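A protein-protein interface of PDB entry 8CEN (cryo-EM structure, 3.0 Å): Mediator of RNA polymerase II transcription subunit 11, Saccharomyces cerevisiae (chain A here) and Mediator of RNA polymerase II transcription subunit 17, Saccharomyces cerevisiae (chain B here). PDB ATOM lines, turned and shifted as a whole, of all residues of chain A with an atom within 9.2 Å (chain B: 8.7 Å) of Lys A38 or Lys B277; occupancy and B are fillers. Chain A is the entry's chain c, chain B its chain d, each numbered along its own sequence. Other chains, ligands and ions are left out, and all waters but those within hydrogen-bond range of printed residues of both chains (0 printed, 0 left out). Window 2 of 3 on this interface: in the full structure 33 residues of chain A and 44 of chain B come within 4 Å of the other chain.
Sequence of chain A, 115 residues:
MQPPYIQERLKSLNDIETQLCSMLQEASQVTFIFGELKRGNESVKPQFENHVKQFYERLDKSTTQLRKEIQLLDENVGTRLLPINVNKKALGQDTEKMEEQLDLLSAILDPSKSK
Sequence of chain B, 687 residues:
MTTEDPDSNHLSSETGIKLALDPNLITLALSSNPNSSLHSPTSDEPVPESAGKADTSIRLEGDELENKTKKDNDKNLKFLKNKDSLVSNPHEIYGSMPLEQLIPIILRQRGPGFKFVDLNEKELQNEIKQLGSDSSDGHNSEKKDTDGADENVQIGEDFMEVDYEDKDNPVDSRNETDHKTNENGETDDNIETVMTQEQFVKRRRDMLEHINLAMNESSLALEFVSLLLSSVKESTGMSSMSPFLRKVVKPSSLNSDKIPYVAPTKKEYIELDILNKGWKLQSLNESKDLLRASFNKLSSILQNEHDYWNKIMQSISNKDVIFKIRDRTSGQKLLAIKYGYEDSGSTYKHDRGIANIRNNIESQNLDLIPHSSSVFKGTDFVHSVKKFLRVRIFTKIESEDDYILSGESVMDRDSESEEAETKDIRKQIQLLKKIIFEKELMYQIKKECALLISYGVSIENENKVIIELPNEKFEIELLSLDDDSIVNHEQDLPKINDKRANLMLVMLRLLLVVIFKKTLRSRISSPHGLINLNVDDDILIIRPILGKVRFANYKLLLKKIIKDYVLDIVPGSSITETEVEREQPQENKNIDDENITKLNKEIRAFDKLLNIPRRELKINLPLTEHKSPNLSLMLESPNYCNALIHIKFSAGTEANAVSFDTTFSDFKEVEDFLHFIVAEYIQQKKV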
ATOM      1  N   VAL A  30      10.563 -32.737   8.053  1.00  0.00           N
ATOM      2  CA  VAL A  30       9.297 -32.630   7.328  1.00  0.00           C
ATOM      3  C   VAL A  30       8.428 -31.529   7.929  1.00  0.00           C
ATOM      4  O   VAL A  30       7.860 -30.701   7.203  1.00  0.00           O
ATOM      5  CB  VAL A  30       8.576 -33.991   7.309  1.00  0.00           C
ATOM      6  CG1 VAL A  30       7.103 -33.828   6.997  1.00  0.00           C
ATOM      7  CG2 VAL A  30       9.214 -34.913   6.284  1.00  0.00           C
ATOM      8  N   THR A  31       8.334 -31.484   9.266  1.00  0.00           N
ATOM      9  CA  THR A  31       7.586 -30.410   9.919  1.00  0.00           C
ATOM     10  C   THR A  31       8.221 -29.043   9.681  1.00  0.00           C
ATOM     11  O   THR A  31       7.499 -28.057   9.502  1.00  0.00           O
ATOM     12  CB  THR A  31       7.456 -30.674  11.421  1.00  0.00           C
ATOM     13  OG1 THR A  31       8.757 -30.732  12.019  1.00  0.00           O
ATOM     14  CG2 THR A  31       6.697 -31.967  11.685  1.00  0.00           C
ATOM     15  N   PHE A  32       9.556 -28.972   9.644  1.00  0.00           N
ATOM     16  CA  PHE A  32      10.240 -27.721   9.314  1.00  0.00           C
ATOM     17  C   PHE A  32       9.871 -27.229   7.922  1.00  0.00           C
ATOM     18  O   PHE A  32       9.449 -26.075   7.750  1.00  0.00           O
ATOM     19  CB  PHE A  32      11.754 -27.916   9.413  1.00  0.00           C
ATOM     20  CG  PHE A  32      12.548 -26.694   9.050  1.00  0.00           C
ATOM     21  CD1 PHE A  32      12.554 -25.586   9.879  1.00  0.00           C
ATOM     22  CD2 PHE A  32      13.288 -26.654   7.879  1.00  0.00           C
ATOM     23  CE1 PHE A  32      13.283 -24.459   9.549  1.00  0.00           C
ATOM     24  CE2 PHE A  32      14.019 -25.528   7.541  1.00  0.00           C
ATOM     25  CZ  PHE A  32      14.015 -24.430   8.379  1.00  0.00           C
ATOM     26  N   ILE A  33      10.012 -28.109   6.923  1.00  0.00           N
ATOM     27  CA  ILE A  33       9.773 -27.739   5.530  1.00  0.00           C
ATOM     28  C   ILE A  33       8.317 -27.341   5.329  1.00  0.00           C
ATOM     29  O   ILE A  33       8.021 -26.347   4.647  1.00  0.00           O
ATOM     30  CB  ILE A  33      10.183 -28.888   4.589  1.00  0.00           C
ATOM     31  CG1 ILE A  33      11.675 -29.226   4.713  1.00  0.00           C
ATOM     32  CG2 ILE A  33       9.872 -28.534   3.160  1.00  0.00           C
ATOM     33  CD1 ILE A  33      12.622 -28.162   4.247  1.00  0.00           C
ATOM     34  N   PHE A  34       7.389 -28.088   5.949  1.00  0.00           N
ATOM     35  CA  PHE A  34       5.992 -27.669   5.976  1.00  0.00           C
ATOM     36  C   PHE A  34       5.838 -26.310   6.641  1.00  0.00           C
ATOM     37  O   PHE A  34       4.977 -25.521   6.238  1.00  0.00           O
ATOM     38  CB  PHE A  34       5.130 -28.707   6.700  1.00  0.00           C
ATOM     39  CG  PHE A  34       3.655 -28.539   6.459  1.00  0.00           C
ATOM     40  CD1 PHE A  34       3.108 -28.806   5.216  1.00  0.00           C
ATOM     41  CD2 PHE A  34       2.818 -28.100   7.471  1.00  0.00           C
ATOM     42  CE1 PHE A  34       1.755 -28.648   4.988  1.00  0.00           C
ATOM     43  CE2 PHE A  34       1.462 -27.939   7.251  1.00  0.00           C
ATOM     44  CZ  PHE A  34       0.931 -28.212   6.006  1.00  0.00           C
ATOM     45  N   GLY A  35       6.692 -26.008   7.624  1.00  0.00           N
ATOM     46  CA  GLY A  35       6.661 -24.698   8.253  1.00  0.00           C
ATOM     47  C   GLY A  35       6.938 -23.560   7.289  1.00  0.00           C
ATOM     48  O   GLY A  35       6.154 -22.610   7.200  1.00  0.00           O
ATOM     49  N   GLU A  36       8.046 -23.638   6.536  1.00  0.00           N
ATOM     50  CA  GLU A  36       8.277 -22.478   5.663  1.00  0.00           C
ATOM     51  C   GLU A  36       7.359 -22.494   4.442  1.00  0.00           C
ATOM     52  O   GLU A  36       7.074 -21.426   3.887  1.00  0.00           O
ATOM     53  CB  GLU A  36       9.721 -22.252   5.165  1.00  0.00           C
ATOM     54  CG  GLU A  36      10.358 -23.202   4.157  1.00  0.00           C
ATOM     55  CD  GLU A  36      11.016 -24.392   4.766  1.00  0.00           C
ATOM     56  OE1 GLU A  36      10.759 -24.662   5.937  1.00  0.00           O
ATOM     57  OE2 GLU A  36      11.813 -25.047   4.068  1.00  0.00           O
ATOM     58  N   LEU A  37       6.868 -23.662   4.003  1.00  0.00           N
ATOM     59  CA  LEU A  37       5.936 -23.590   2.879  1.00  0.00           C
ATOM     60  C   LEU A  37       4.533 -23.162   3.304  1.00  0.00           C
ATOM     61  O   LEU A  37       3.752 -22.733   2.450  1.00  0.00           O
ATOM     62  CB  LEU A  37       5.882 -24.908   2.094  1.00  0.00           C
ATOM     63  CG  LEU A  37       5.502 -26.276   2.654  1.00  0.00           C
ATOM     64  CD1 LEU A  37       4.013 -26.515   2.650  1.00  0.00           C
ATOM     65  CD2 LEU A  37       6.207 -27.361   1.866  1.00  0.00           C
ATOM     66  N   LYS A  38       4.193 -23.262   4.593  1.00  0.00           N
ATOM     67  CA  LYS A  38       3.014 -22.556   5.087  1.00  0.00           C
ATOM     68  C   LYS A  38       3.288 -21.075   5.294  1.00  0.00           C
ATOM     69  O   LYS A  38       2.365 -20.260   5.180  1.00  0.00           O
ATOM     70  CB  LYS A  38       2.507 -23.174   6.390  1.00  0.00           C
ATOM     71  CG  LYS A  38       1.937 -24.567   6.250  1.00  0.00           C
ATOM     72  CD  LYS A  38       0.708 -24.558   5.372  1.00  0.00           C
ATOM     73  CE  LYS A  38      -0.412 -23.792   6.045  1.00  0.00           C
ATOM     74  NZ  LYS A  38      -0.878 -24.435   7.296  1.00  0.00           N
ATOM     75  N   ARG A  39       4.532 -20.710   5.624  1.00  0.00           N
ATOM     76  CA  ARG A  39       4.895 -19.296   5.636  1.00  0.00           C
ATOM     77  C   ARG A  39       4.793 -18.676   4.247  1.00  0.00           C
ATOM     78  O   ARG A  39       4.485 -17.485   4.122  1.00  0.00           O
ATOM     79  CB  ARG A  39       6.304 -19.099   6.196  1.00  0.00           C
ATOM     80  CG  ARG A  39       6.449 -19.415   7.671  1.00  0.00           C
ATOM     81  CD  ARG A  39       7.873 -19.156   8.129  1.00  0.00           C
ATOM     82  NE  ARG A  39       8.078 -19.520   9.525  1.00  0.00           N
ATOM     83  CZ  ARG A  39       7.879 -18.695  10.542  1.00  0.00           C
ATOM     84  NH1 ARG A  39       7.451 -17.458  10.355  1.00  0.00           N
ATOM     85  NH2 ARG A  39       8.118 -19.119  11.779  1.00  0.00           N
ATOM     86  N   GLY A  40       5.040 -19.456   3.197  1.00  0.00           N
ATOM     87  CA  GLY A  40       4.802 -18.962   1.854  1.00  0.00           C
ATOM     88  C   GLY A  40       5.835 -19.331   0.810  1.00  0.00           C
ATOM     89  O   GLY A  40       5.647 -19.036  -0.375  1.00  0.00           O
ATOM     90  N   ASN A  41       6.928 -19.965   1.224  1.00  0.00           N
ATOM     91  CA  ASN A  41       7.954 -20.372   0.274  1.00  0.00           C
ATOM     92  C   ASN A  41       7.457 -21.536  -0.576  1.00  0.00           C
ATOM     93  O   ASN A  41       6.848 -22.481  -0.069  1.00  0.00           O
ATOM     94  CB  ASN A  41       9.234 -20.761   1.011  1.00  0.00           C
ATOM     95  CG  ASN A  41      10.452 -20.735   0.112  1.00  0.00           C
ATOM     96  OD1 ASN A  41      10.357 -20.407  -1.071  1.00  0.00           O
ATOM     97  ND2 ASN A  41      11.606 -21.082   0.669  1.00  0.00           N
ATOM     98  N   GLU A  42       7.716 -21.463  -1.882  1.00  0.00           N
ATOM     99  CA  GLU A  42       7.243 -22.475  -2.817  1.00  0.00           C
ATOM    100  C   GLU A  42       8.354 -23.246  -3.515  1.00  0.00           C
ATOM    101  O   GLU A  42       8.074 -24.298  -4.100  1.00  0.00           O
ATOM    102  CB  GLU A  42       6.339 -21.839  -3.884  1.00  0.00           C
ATOM    103  CG  GLU A  42       4.992 -21.361  -3.361  1.00  0.00           C
ATOM    104  CD  GLU A  42       3.951 -22.461  -3.339  1.00  0.00           C
ATOM    105  OE1 GLU A  42       4.004 -23.316  -2.429  1.00  0.00           O
ATOM    106  OE2 GLU A  42       3.082 -22.475  -4.236  1.00  0.00           O
ATOM    107  N   VAL A  44      10.732 -24.949  -2.253  1.00  0.00           N
ATOM    108  CA  VAL A  44      11.219 -26.065  -1.452  1.00  0.00           C
ATOM    109  C   VAL A  44      10.208 -27.227  -1.482  1.00  0.00           C
ATOM    110  O   VAL A  44      10.402 -28.270  -0.843  1.00  0.00           O
ATOM    111  CB  VAL A  44      11.551 -25.521  -0.037  1.00  0.00           C
ATOM    112  CG1 VAL A  44      12.018 -26.551   0.998  1.00  0.00           C
ATOM    113  CG2 VAL A  44      12.566 -24.387  -0.143  1.00  0.00           C
ATOM    114  N   PHE A  48      10.110 -31.020   0.150  1.00  0.00           N
ATOM    115  CA  PHE A  48       9.057 -31.547   1.019  1.00  0.00           C
ATOM    116  C   PHE A  48       8.616 -32.929   0.561  1.00  0.00           C
ATOM    117  O   PHE A  48       8.476 -33.855   1.375  1.00  0.00           O
ATOM    118  CB  PHE A  48       7.861 -30.593   1.039  1.00  0.00           C
ATOM    119  CG  PHE A  48       6.677 -31.113   1.812  1.00  0.00           C
ATOM    120  CD1 PHE A  48       6.640 -31.009   3.193  1.00  0.00           C
ATOM    121  CD2 PHE A  48       5.588 -31.673   1.158  1.00  0.00           C
ATOM    122  CE1 PHE A  48       5.554 -31.477   3.911  1.00  0.00           C
ATOM    123  CE2 PHE A  48       4.499 -32.143   1.871  1.00  0.00           C
ATOM    124  CZ  PHE A  48       4.482 -32.042   3.248  1.00  0.00           C
ATOM    125  N   ILE B 270     -11.914 -13.997   8.496  1.00  0.00           N
ATOM    126  CA  ILE B 270     -10.521 -13.994   8.057  1.00  0.00           C
ATOM    127  C   ILE B 270      -9.590 -13.659   9.218  1.00  0.00           C
ATOM    128  O   ILE B 270      -8.433 -14.086   9.224  1.00  0.00           O
ATOM    129  CB  ILE B 270     -10.306 -13.052   6.855  1.00  0.00           C
ATOM    130  CG1 ILE B 270     -10.623 -11.601   7.209  1.00  0.00           C
ATOM    131  CG2 ILE B 270     -11.142 -13.508   5.666  1.00  0.00           C
ATOM    132  CD1 ILE B 270     -10.212 -10.610   6.148  1.00  0.00           C
ATOM    133  N   GLU B 271     -10.081 -12.943  10.237  1.00  0.00           N
ATOM    134  CA  GLU B 271      -9.267 -12.714  11.429  1.00  0.00           C
ATOM    135  C   GLU B 271      -9.050 -14.006  12.213  1.00  0.00           C
ATOM    136  O   GLU B 271      -7.921 -14.311  12.622  1.00  0.00           O
ATOM    137  CB  GLU B 271      -9.923 -11.651  12.311  1.00  0.00           C
ATOM    138  CG  GLU B 271      -9.111 -11.263  13.537  1.00  0.00           C
ATOM    139  CD  GLU B 271      -7.854 -10.487  13.185  1.00  0.00           C
ATOM    140  OE1 GLU B 271      -7.845  -9.806  12.137  1.00  0.00           O
ATOM    141  OE2 GLU B 271      -6.874 -10.555  13.956  1.00  0.00           O
ATOM    142  N   LEU B 272     -10.114 -14.789  12.415  1.00  0.00           N
ATOM    143  CA  LEU B 272      -9.972 -16.087  13.065  1.00  0.00           C
ATOM    144  C   LEU B 272      -9.129 -17.034  12.219  1.00  0.00           C
ATOM    145  O   LEU B 272      -8.348 -17.826  12.755  1.00  0.00           O
ATOM    146  CB  LEU B 272     -11.355 -16.677  13.338  1.00  0.00           C
ATOM    147  CG  LEU B 272     -11.458 -18.150  13.731  1.00  0.00           C
ATOM    148  CD1 LEU B 272     -10.952 -18.365  15.148  1.00  0.00           C
ATOM    149  CD2 LEU B 272     -12.887 -18.635  13.581  1.00  0.00           C
ATOM    150  N   ASP B 273      -9.252 -16.940  10.892  1.00  0.00           N
ATOM    151  CA  ASP B 273      -8.484 -17.799   9.997  1.00  0.00           C
ATOM    152  C   ASP B 273      -6.996 -17.469  10.039  1.00  0.00           C
ATOM    153  O   ASP B 273      -6.157 -18.375  10.064  1.00  0.00           O
ATOM    154  CB  ASP B 273      -9.026 -17.668   8.575  1.00  0.00           C
ATOM    155  CG  ASP B 273     -10.191 -18.603   8.308  1.00  0.00           C
ATOM    156  OD1 ASP B 273     -10.643 -19.280   9.255  1.00  0.00           O
ATOM    157  OD2 ASP B 273     -10.657 -18.661   7.150  1.00  0.00           O
ATOM    158  N   ILE B 274      -6.643 -16.179  10.049  1.00  0.00           N
ATOM    159  CA  ILE B 274      -5.233 -15.805  10.095  1.00  0.00           C
ATOM    160  C   ILE B 274      -4.651 -16.105  11.474  1.00  0.00           C
ATOM    161  O   ILE B 274      -3.476 -16.489  11.593  1.00  0.00           O
ATOM    162  CB  ILE B 274      -5.061 -14.330   9.660  1.00  0.00           C
ATOM    163  CG1 ILE B 274      -3.603 -13.986   9.397  1.00  0.00           C
ATOM    164  CG2 ILE B 274      -5.597 -13.341  10.678  1.00  0.00           C
ATOM    165  CD1 ILE B 274      -3.469 -12.670   8.672  1.00  0.00           C
ATOM    166  N   LEU B 275      -5.475 -15.997  12.527  1.00  0.00           N
ATOM    167  CA  LEU B 275      -5.080 -16.457  13.854  1.00  0.00           C
ATOM    168  C   LEU B 275      -4.794 -17.952  13.861  1.00  0.00           C
ATOM    169  O   LEU B 275      -3.794 -18.400  14.438  1.00  0.00           O
ATOM    170  CB  LEU B 275      -6.191 -16.128  14.847  1.00  0.00           C
ATOM    171  CG  LEU B 275      -6.152 -16.711  16.256  1.00  0.00           C
ATOM    172  CD1 LEU B 275      -4.939 -16.219  17.025  1.00  0.00           C
ATOM    173  CD2 LEU B 275      -7.449 -16.375  16.972  1.00  0.00           C
ATOM    174  N   ASN B 276      -5.666 -18.734  13.218  1.00  0.00           N
ATOM    175  CA  ASN B 276      -5.476 -20.176  13.125  1.00  0.00           C
ATOM    176  C   ASN B 276      -4.202 -20.516  12.366  1.00  0.00           C
ATOM    177  O   ASN B 276      -3.443 -21.394  12.787  1.00  0.00           O
ATOM    178  CB  ASN B 276      -6.689 -20.811  12.446  1.00  0.00           C
ATOM    179  CG  ASN B 276      -6.682 -22.324  12.527  1.00  0.00           C
ATOM    180  OD1 ASN B 276      -5.908 -22.918  13.275  1.00  0.00           O
ATOM    181  ND2 ASN B 276      -7.555 -22.957  11.753  1.00  0.00           N
ATOM    182  N   LYS B 277      -3.948 -19.815  11.258  1.00  0.00           N
ATOM    183  CA  LYS B 277      -2.750 -20.066  10.461  1.00  0.00           C
ATOM    184  C   LYS B 277      -1.484 -19.785  11.261  1.00  0.00           C
ATOM    185  O   LYS B 277      -0.569 -20.619  11.312  1.00  0.00           O
ATOM    186  CB  LYS B 277      -2.787 -19.212   9.192  1.00  0.00           C
ATOM    187  CG  LYS B 277      -1.492 -19.215   8.397  1.00  0.00           C
ATOM    188  CD  LYS B 277      -1.688 -18.578   7.030  1.00  0.00           C
ATOM    189  CE  LYS B 277      -0.380 -18.503   6.262  1.00  0.00           C
ATOM    190  NZ  LYS B 277       0.587 -17.563   6.892  1.00  0.00           N
ATOM    191  N   GLY B 278      -1.433 -18.630  11.930  1.00  0.00           N
ATOM    192  CA  GLY B 278      -0.258 -18.298  12.721  1.00  0.00           C
ATOM    193  C   GLY B 278      -0.052 -19.223  13.906  1.00  0.00           C
ATOM    194  O   GLY B 278       1.083 -19.594  14.226  1.00  0.00           O
ATOM    195  N   TRP B 279      -1.140 -19.632  14.559  1.00  0.00           N
ATOM    196  CA  TRP B 279      -0.982 -20.430  15.765  1.00  0.00           C
ATOM    197  C   TRP B 279      -0.625 -21.869  15.394  1.00  0.00           C
ATOM    198  O   TRP B 279       0.177 -22.513  16.083  1.00  0.00           O
ATOM    199  CB  TRP B 279      -2.264 -20.336  16.600  1.00  0.00           C
ATOM    200  CG  TRP B 279      -2.168 -20.814  18.029  1.00  0.00           C
ATOM    201  CD1 TRP B 279      -1.307 -21.731  18.549  1.00  0.00           C
ATOM    202  CD2 TRP B 279      -2.938 -20.325  19.132  1.00  0.00           C
ATOM    203  NE1 TRP B 279      -1.512 -21.869  19.898  1.00  0.00           N
ATOM    204  CE2 TRP B 279      -2.508 -21.013  20.281  1.00  0.00           C
ATOM    205  CE3 TRP B 279      -3.958 -19.381  19.253  1.00  0.00           C
ATOM    206  CZ2 TRP B 279      -3.064 -20.787  21.533  1.00  0.00           C
ATOM    207  CZ3 TRP B 279      -4.509 -19.162  20.494  1.00  0.00           C
ATOM    208  CH2 TRP B 279      -4.054 -19.852  21.620  1.00  0.00           C
ATOM    209  N   LYS B 280      -1.172 -22.374  14.280  1.00  0.00           N
ATOM    210  CA  LYS B 280      -0.748 -23.670  13.759  1.00  0.00           C
ATOM    211  C   LYS B 280       0.715 -23.643  13.332  1.00  0.00           C
ATOM    212  O   LYS B 280       1.436 -24.628  13.517  1.00  0.00           O
ATOM    213  CB  LYS B 280      -1.634 -24.091  12.586  1.00  0.00           C
ATOM    214  CG  LYS B 280      -3.037 -24.558  12.952  1.00  0.00           C
ATOM    215  CD  LYS B 280      -3.026 -25.643  14.008  1.00  0.00           C
ATOM    216  CE  LYS B 280      -4.430 -25.918  14.519  1.00  0.00           C
ATOM    217  NZ  LYS B 280      -5.425 -25.960  13.410  1.00  0.00           N
ATOM    218  N   LEU B 281       1.171 -22.522  12.760  1.00  0.00           N
ATOM    219  CA  LEU B 281       2.589 -22.388  12.429  1.00  0.00           C
ATOM    220  C   LEU B 281       3.463 -22.413  13.679  1.00  0.00           C
ATOM    221  O   LEU B 281       4.540 -23.024  13.681  1.00  0.00           O
ATOM    222  CB  LEU B 281       2.822 -21.103  11.637  1.00  0.00           C
ATOM    223  CG  LEU B 281       2.699 -21.237  10.122  1.00  0.00           C
ATOM    224  CD1 LEU B 281       2.591 -19.874   9.462  1.00  0.00           C
ATOM    225  CD2 LEU B 281       3.898 -21.999   9.592  1.00  0.00           C
ATOM    226  N   GLN B 282       3.021 -21.745  14.749  1.00  0.00           N
ATOM    227  CA  GLN B 282       3.782 -21.762  15.997  1.00  0.00           C
ATOM    228  C   GLN B 282       3.832 -23.162  16.603  1.00  0.00           C
ATOM    229  O   GLN B 282       4.877 -23.589  17.114  1.00  0.00           O
ATOM    230  CB  GLN B 282       3.185 -20.766  16.991  1.00  0.00           C
ATOM    231  CG  GLN B 282       4.060 -20.506  18.207  1.00  0.00           C
ATOM    232  CD  GLN B 282       5.467 -20.075  17.836  1.00  0.00           C
ATOM    233  OE1 GLN B 282       5.662 -19.229  16.962  1.00  0.00           O
ATOM    234  NE2 GLN B 282       6.456 -20.658  18.502  1.00  0.00           N
ATOM    235  N   SER B 283       2.715 -23.895  16.545  1.00  0.00           N
ATOM    236  CA  SER B 283       2.709 -25.277  17.019  1.00  0.00           C
ATOM    237  C   SER B 283       3.598 -26.169  16.163  1.00  0.00           C
ATOM    238  O   SER B 283       4.244 -27.082  16.687  1.00  0.00           O
ATOM    239  CB  SER B 283       1.286 -25.827  17.041  1.00  0.00           C
ATOM    240  OG  SER B 283       0.738 -25.879  15.738  1.00  0.00           O
ATOM    241  N   LEU B 284       3.644 -25.913  14.852  1.00  0.00           N
ATOM    242  CA  LEU B 284       4.545 -26.650  13.971  1.00  0.00           C
ATOM    243  C   LEU B 284       6.002 -26.392  14.328  1.00  0.00           C
ATOM    244  O   LEU B 284       6.820 -27.318  14.326  1.00  0.00           O
ATOM    245  CB  LEU B 284       4.276 -26.257  12.520  1.00  0.00           C
ATOM    246  CG  LEU B 284       3.112 -26.957  11.825  1.00  0.00           C
ATOM    247  CD1 LEU B 284       2.823 -26.268  10.512  1.00  0.00           C
ATOM    248  CD2 LEU B 284       3.433 -28.425  11.603  1.00  0.00           C
ATOM    249  N   ASN B 285       6.343 -25.137  14.635  1.00  0.00           N
ATOM    250  CA  ASN B 285       7.709 -24.818  15.046  1.00  0.00           C
ATOM    251  C   ASN B 285       8.065 -25.490  16.367  1.00  0.00           C
ATOM    252  O   ASN B 285       9.183 -26.000  16.533  1.00  0.00           O
ATOM    253  CB  ASN B 285       7.887 -23.305  15.155  1.00  0.00           C
ATOM    254  CG  ASN B 285       8.046 -22.640  13.807  1.00  0.00           C
ATOM    255  OD1 ASN B 285       7.661 -21.486  13.620  1.00  0.00           O
ATOM    256  ND2 ASN B 285       8.616 -23.367  12.854  1.00  0.00           N
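Of chain B, only Lys B277 and Leu B281 come within 4 Å of Lys A38.
Lys B277 touches one residue of chain A.
No residue of chain A comes within 4 Å of Asn B276.
Printed residues of chain B within 4 Å of Arg A39: Asn B285 (3.0 Å).
Of the printed residues of chain B, Phe A34 touches Leu B284.
The nearest printed residue of chain A that does not touch Leu B281 is Arg A39 (4.1 Å).
The backbone carbonyl oxygen of Leu B281 sits close to the side-chain amide oxygen of Asn B285.
NH2 of Arg A39 is in hydrogen-bond range of OD1 of Asn B285 (3.0 Å).
Among the printed residues, pairs that only touch across the chains: Gly A35 with Leu B281 (3.3 Å), Lys A38 with Lys B277 (3.4 Å), Phe A34 with Leu B284 (3.6 Å) and Lys A38 with Leu B281 (3.7 Å).
Of the 15 printed residues of chain A, 4 touch a printed residue of chain B.
Printed residues of chain A that touch a printed residue of chain B: Phe A34, Gly A35, Lys A38 and Arg A39.
Hydrophobic or aromatic side chains of chain A within 4 Å of the printed part of chain B: Phe A34.
Of the 16 printed residues of chain B, 4 touch a printed residue of chain A.
Among the printed residues, 5 pairs touch across the chains.
Among the printed residues, no Asp or Glu carboxylate lies within 4 Å of a Lys or Arg side-chain nitrogen of the other chain.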
